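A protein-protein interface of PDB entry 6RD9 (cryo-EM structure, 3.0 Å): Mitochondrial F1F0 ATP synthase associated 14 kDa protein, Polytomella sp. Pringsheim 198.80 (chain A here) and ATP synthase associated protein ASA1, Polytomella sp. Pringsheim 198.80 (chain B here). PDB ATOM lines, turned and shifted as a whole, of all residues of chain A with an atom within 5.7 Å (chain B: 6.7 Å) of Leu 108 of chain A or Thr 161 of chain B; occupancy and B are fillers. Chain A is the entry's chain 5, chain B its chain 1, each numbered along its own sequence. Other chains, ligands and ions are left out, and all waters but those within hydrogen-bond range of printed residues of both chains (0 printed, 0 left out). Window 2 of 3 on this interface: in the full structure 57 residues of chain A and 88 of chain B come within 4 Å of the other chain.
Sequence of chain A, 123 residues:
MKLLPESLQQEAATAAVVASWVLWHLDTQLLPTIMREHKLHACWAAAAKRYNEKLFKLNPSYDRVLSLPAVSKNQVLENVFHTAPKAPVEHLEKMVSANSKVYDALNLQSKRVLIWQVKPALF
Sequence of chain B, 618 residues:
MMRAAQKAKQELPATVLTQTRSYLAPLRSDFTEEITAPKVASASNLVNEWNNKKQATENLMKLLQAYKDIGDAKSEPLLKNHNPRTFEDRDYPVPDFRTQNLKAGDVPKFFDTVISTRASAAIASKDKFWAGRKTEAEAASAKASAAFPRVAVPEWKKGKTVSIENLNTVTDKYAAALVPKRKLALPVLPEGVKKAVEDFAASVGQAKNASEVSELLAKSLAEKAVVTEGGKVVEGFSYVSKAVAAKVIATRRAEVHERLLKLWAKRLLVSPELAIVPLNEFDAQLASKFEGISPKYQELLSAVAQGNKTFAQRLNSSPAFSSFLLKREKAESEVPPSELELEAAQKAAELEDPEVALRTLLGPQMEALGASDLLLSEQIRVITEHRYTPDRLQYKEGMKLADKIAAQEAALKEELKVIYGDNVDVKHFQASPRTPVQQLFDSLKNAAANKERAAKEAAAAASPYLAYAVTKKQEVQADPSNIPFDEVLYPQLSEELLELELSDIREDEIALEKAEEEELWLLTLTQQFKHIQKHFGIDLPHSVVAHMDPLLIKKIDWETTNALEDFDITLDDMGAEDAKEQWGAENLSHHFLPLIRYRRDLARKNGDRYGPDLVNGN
Of chain B, only Thr 161 comes within 4 Å of Leu 108 of chain A. Ile 115 of chain A touches none of the printed residues of chain B. Glu 155 of chain B touches none of the printed residues of chain A. Printed residues of chain A within 4 Å of Trp 156 of chain B: Leu 106. Thr 161 of chain B touches just these residues of chain A: Leu 106 and Leu 108. Of the printed residues of chain A, Val 162 of chain B touches Leu 106 and Asn 107. Printed residues of chain A within 4 Å of Ser 163 of chain B: Asn 107. The nearest residue of chain A that does not touch Thr 161 of chain B is Asn 107 of chain A (4.1 Å).
Leu 106 of chain A touches Trp 156 of chain B. Leu 106 of chain A touches Thr 161 of chain B. Ser 163 of chain B touches Asn 107 of chain A (C to OD1, 3.9 Å). CG of Leu 108 of chain A touches CG2 of Thr 161 of chain B, at 3.7 Å.
The backbone carbonyl oxygen (O) of Leu 106 of chain A is in hydrogen-bond range of the backbone NH (N) of Val 162 of chain B (2.7 Å). The side-chain amide oxygen (OD1) of Asn 107 of chain A lies close to the backbone carbonyl oxygen (O) of Val 162 of chain B (2.8 Å).
Of the 8 printed residues of chain B, 4 touch a printed residue of chain A. Hydrophobic or aromatic side chains of chain B that line the printed part of chain A: Trp 156 and Val 162. Hydrophobic or aromatic side chains of chain A within 4 Å of the printed part of chain B: Leu 106 and Leu 108. Among the printed residues, 6 pairs touch across the chains.
ND2 of Asn 107 of chain A sits close to N of Gln 109 of chain A.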
ATOM      1  N   TYR A 103       3.598  -7.809  -1.947  1.00  0.00           N
ATOM      2  CA  TYR A 103       4.280  -8.624  -0.954  1.00  0.00           C
ATOM      3  C   TYR A 103       4.878  -7.755   0.120  1.00  0.00           C
ATOM      4  O   TYR A 103       4.787  -8.094   1.298  1.00  0.00           O
ATOM      5  CB  TYR A 103       5.386  -9.473  -1.573  1.00  0.00           C
ATOM      6  CG  TYR A 103       6.161 -10.275  -0.549  1.00  0.00           C
ATOM      7  CD1 TYR A 103       5.659 -11.441  -0.049  1.00  0.00           C
ATOM      8  CD2 TYR A 103       7.391  -9.852  -0.077  1.00  0.00           C
ATOM      9  CE1 TYR A 103       6.343 -12.160   0.862  1.00  0.00           C
ATOM     10  CE2 TYR A 103       8.057 -10.561   0.863  1.00  0.00           C
ATOM     11  CZ  TYR A 103       7.530 -11.713   1.320  1.00  0.00           C
ATOM     12  OH  TYR A 103       8.197 -12.442   2.254  1.00  0.00           O
ATOM     13  N   LEU A 106       2.170  -6.007   2.494  1.00  0.00           N
ATOM     14  CA  LEU A 106       0.995  -6.667   3.040  1.00  0.00           C
ATOM     15  C   LEU A 106       1.230  -8.121   3.386  1.00  0.00           C
ATOM     16  O   LEU A 106       0.305  -8.927   3.296  1.00  0.00           O
ATOM     17  CB  LEU A 106      -0.157  -6.615   2.056  1.00  0.00           C
ATOM     18  CG  LEU A 106      -0.630  -5.320   1.457  1.00  0.00           C
ATOM     19  CD1 LEU A 106      -1.482  -5.692   0.318  1.00  0.00           C
ATOM     20  CD2 LEU A 106      -1.427  -4.572   2.443  1.00  0.00           C
ATOM     21  N   ASN A 107       2.415  -8.507   3.835  1.00  0.00           N
ATOM     22  CA  ASN A 107       2.625  -9.945   3.965  1.00  0.00           C
ATOM     23  C   ASN A 107       2.609 -10.501   5.373  1.00  0.00           C
ATOM     24  O   ASN A 107       2.022 -11.568   5.568  1.00  0.00           O
ATOM     25  CB  ASN A 107       3.933 -10.381   3.349  1.00  0.00           C
ATOM     26  CG  ASN A 107       3.982 -11.856   3.154  1.00  0.00           C
ATOM     27  OD1 ASN A 107       3.352 -12.385   2.264  1.00  0.00           O
ATOM     28  ND2 ASN A 107       4.757 -12.533   3.968  1.00  0.00           N
ATOM     29  N   LEU A 108       3.234  -9.803   6.328  1.00  0.00           N
ATOM     30  CA  LEU A 108       3.592 -10.101   7.733  1.00  0.00           C
ATOM     31  C   LEU A 108       4.954 -10.750   7.872  1.00  0.00           C
ATOM     32  O   LEU A 108       5.399 -10.921   8.989  1.00  0.00           O
ATOM     33  CB  LEU A 108       2.608 -10.986   8.511  1.00  0.00           C
ATOM     34  CG  LEU A 108       1.228 -10.374   8.641  1.00  0.00           C
ATOM     35  CD1 LEU A 108       0.256 -11.338   9.293  1.00  0.00           C
ATOM     36  CD2 LEU A 108       1.340  -9.092   9.423  1.00  0.00           C
ATOM     37  N   GLN A 109       5.634 -11.094   6.797  1.00  0.00           N
ATOM     38  CA  GLN A 109       7.020 -11.504   6.902  1.00  0.00           C
ATOM     39  C   GLN A 109       7.948 -10.582   6.149  1.00  0.00           C
ATOM     40  O   GLN A 109       9.151 -10.833   6.124  1.00  0.00           O
ATOM     41  CB  GLN A 109       7.234 -12.930   6.391  1.00  0.00           C
ATOM     42  CG  GLN A 109       7.083 -14.017   7.422  1.00  0.00           C
ATOM     43  CD  GLN A 109       5.657 -14.377   7.675  1.00  0.00           C
ATOM     44  OE1 GLN A 109       5.167 -14.269   8.794  1.00  0.00           O
ATOM     45  NE2 GLN A 109       4.970 -14.816   6.635  1.00  0.00           N
ATOM     46  N   SER A 110       7.430  -9.537   5.535  1.00  0.00           N
ATOM     47  CA  SER A 110       8.258  -8.625   4.784  1.00  0.00           C
ATOM     48  C   SER A 110       9.039  -7.722   5.715  1.00  0.00           C
ATOM     49  O   SER A 110       8.663  -7.500   6.848  1.00  0.00           O
ATOM     50  CB  SER A 110       7.396  -7.792   3.867  1.00  0.00           C
ATOM     51  OG  SER A 110       8.162  -6.781   3.261  1.00  0.00           O
ATOM     52  N   VAL A 113       6.490  -3.990   6.293  1.00  0.00           N
ATOM     53  CA  VAL A 113       5.067  -4.282   6.296  1.00  0.00           C
ATOM     54  C   VAL A 113       4.366  -3.004   6.688  1.00  0.00           C
ATOM     55  O   VAL A 113       4.924  -2.184   7.418  1.00  0.00           O
ATOM     56  CB  VAL A 113       4.702  -5.401   7.281  1.00  0.00           C
ATOM     57  CG1 VAL A 113       3.436  -6.072   6.868  1.00  0.00           C
ATOM     58  CG2 VAL A 113       5.742  -6.350   7.402  1.00  0.00           C
ATOM     59  N   ILE A 115       1.709  -3.157   8.542  1.00  0.00           N
ATOM     60  CA  ILE A 115       0.779  -3.506   9.604  1.00  0.00           C
ATOM     61  C   ILE A 115       1.082  -2.752  10.886  1.00  0.00           C
ATOM     62  O   ILE A 115       0.189  -2.548  11.705  1.00  0.00           O
ATOM     63  CB  ILE A 115       0.765  -5.033   9.804  1.00  0.00           C
ATOM     64  CG1 ILE A 115      -0.423  -5.479  10.640  1.00  0.00           C
ATOM     65  CG2 ILE A 115       2.023  -5.510  10.441  1.00  0.00           C
ATOM     66  CD1 ILE A 115      -1.722  -5.160  10.015  1.00  0.00           C
ATOM     67  N   GLU B 155      -4.945 -12.408  -3.979  1.00  0.00           N
ATOM     68  CA  GLU B 155      -6.164 -12.146  -3.235  1.00  0.00           C
ATOM     69  C   GLU B 155      -5.848 -11.344  -1.988  1.00  0.00           C
ATOM     70  O   GLU B 155      -5.023 -11.752  -1.170  1.00  0.00           O
ATOM     71  CB  GLU B 155      -6.835 -13.455  -2.860  1.00  0.00           C
ATOM     72  CG  GLU B 155      -8.176 -13.282  -2.234  1.00  0.00           C
ATOM     73  CD  GLU B 155      -8.481 -14.375  -1.248  1.00  0.00           C
ATOM     74  OE1 GLU B 155      -7.549 -14.824  -0.557  1.00  0.00           O
ATOM     75  OE2 GLU B 155      -9.648 -14.802  -1.171  1.00  0.00           O
ATOM     76  N   TRP B 156      -6.500 -10.199  -1.854  1.00  0.00           N
ATOM     77  CA  TRP B 156      -6.297  -9.285  -0.749  1.00  0.00           C
ATOM     78  C   TRP B 156      -7.665  -8.926  -0.211  1.00  0.00           C
ATOM     79  O   TRP B 156      -8.478  -8.351  -0.934  1.00  0.00           O
ATOM     80  CB  TRP B 156      -5.548  -8.041  -1.208  1.00  0.00           C
ATOM     81  CG  TRP B 156      -5.304  -7.048  -0.158  1.00  0.00           C
ATOM     82  CD1 TRP B 156      -5.166  -7.282   1.159  1.00  0.00           C
ATOM     83  CD2 TRP B 156      -5.155  -5.644  -0.332  1.00  0.00           C
ATOM     84  NE1 TRP B 156      -4.954  -6.119   1.827  1.00  0.00           N
ATOM     85  CE2 TRP B 156      -4.940  -5.094   0.925  1.00  0.00           C
ATOM     86  CE3 TRP B 156      -5.181  -4.800  -1.433  1.00  0.00           C
ATOM     87  CZ2 TRP B 156      -4.755  -3.749   1.115  1.00  0.00           C
ATOM     88  CZ3 TRP B 156      -4.998  -3.472  -1.241  1.00  0.00           C
ATOM     89  CH2 TRP B 156      -4.783  -2.955   0.018  1.00  0.00           C
ATOM     90  N   LYS B 157      -7.923  -9.280   1.039  1.00  0.00           N
ATOM     91  CA  LYS B 157      -9.177  -8.957   1.690  1.00  0.00           C
ATOM     92  C   LYS B 157      -9.053  -7.585   2.338  1.00  0.00           C
ATOM     93  O   LYS B 157      -8.024  -6.927   2.214  1.00  0.00           O
ATOM     94  CB  LYS B 157      -9.527 -10.045   2.681  1.00  0.00           C
ATOM     95  CG  LYS B 157      -9.688 -11.391   2.059  1.00  0.00           C
ATOM     96  CD  LYS B 157     -10.784 -11.339   1.048  1.00  0.00           C
ATOM     97  CE  LYS B 157     -11.331 -12.699   0.768  1.00  0.00           C
ATOM     98  NZ  LYS B 157     -12.633 -12.558   0.076  1.00  0.00           N
ATOM     99  N   GLY B 159      -9.206  -6.022   5.622  1.00  0.00           N
ATOM    100  CA  GLY B 159      -8.251  -5.744   6.665  1.00  0.00           C
ATOM    101  C   GLY B 159      -7.208  -6.814   6.824  1.00  0.00           C
ATOM    102  O   GLY B 159      -6.431  -6.766   7.786  1.00  0.00           O
ATOM    103  N   LYS B 160      -7.156  -7.777   5.930  1.00  0.00           N
ATOM    104  CA  LYS B 160      -6.311  -8.935   6.116  1.00  0.00           C
ATOM    105  C   LYS B 160      -4.958  -8.684   5.479  1.00  0.00           C
ATOM    106  O   LYS B 160      -4.617  -7.565   5.097  1.00  0.00           O
ATOM    107  CB  LYS B 160      -7.001 -10.159   5.547  1.00  0.00           C
ATOM    108  CG  LYS B 160      -8.376 -10.362   6.095  1.00  0.00           C
ATOM    109  CD  LYS B 160      -8.339 -10.498   7.580  1.00  0.00           C
ATOM    110  CE  LYS B 160      -9.723 -10.483   8.152  1.00  0.00           C
ATOM    111  NZ  LYS B 160      -9.651 -10.457   9.622  1.00  0.00           N
ATOM    112  N   THR B 161      -4.165  -9.730   5.380  1.00  0.00           N
ATOM    113  CA  THR B 161      -2.883  -9.664   4.723  1.00  0.00           C
ATOM    114  C   THR B 161      -2.890 -10.604   3.536  1.00  0.00           C
ATOM    115  O   THR B 161      -3.889 -11.250   3.225  1.00  0.00           O
ATOM    116  CB  THR B 161      -1.760 -10.017   5.683  1.00  0.00           C
ATOM    117  OG1 THR B 161      -2.126 -11.192   6.406  1.00  0.00           O
ATOM    118  CG2 THR B 161      -1.542  -8.883   6.641  1.00  0.00           C
ATOM    119  N   VAL B 162      -1.759 -10.651   2.853  1.00  0.00           N
ATOM    120  CA  VAL B 162      -1.603 -11.440   1.646  1.00  0.00           C
ATOM    121  C   VAL B 162      -0.590 -12.526   1.945  1.00  0.00           C
ATOM    122  O   VAL B 162       0.535 -12.232   2.351  1.00  0.00           O
ATOM    123  CB  VAL B 162      -1.167 -10.565   0.466  1.00  0.00           C
ATOM    124  CG1 VAL B 162      -0.936 -11.397  -0.701  1.00  0.00           C
ATOM    125  CG2 VAL B 162      -2.239  -9.592   0.134  1.00  0.00           C
ATOM    126  N   SER B 163      -0.989 -13.778   1.781  1.00  0.00           N
ATOM    127  CA  SER B 163      -0.093 -14.889   2.032  1.00  0.00           C
ATOM    128  C   SER B 163       0.845 -15.071   0.863  1.00  0.00           C
ATOM    129  O   SER B 163       0.516 -14.750  -0.272  1.00  0.00           O
ATOM    130  CB  SER B 163      -0.880 -16.171   2.262  1.00  0.00           C
ATOM    131  OG  SER B 163      -1.789 -16.388   1.207  1.00  0.00           O
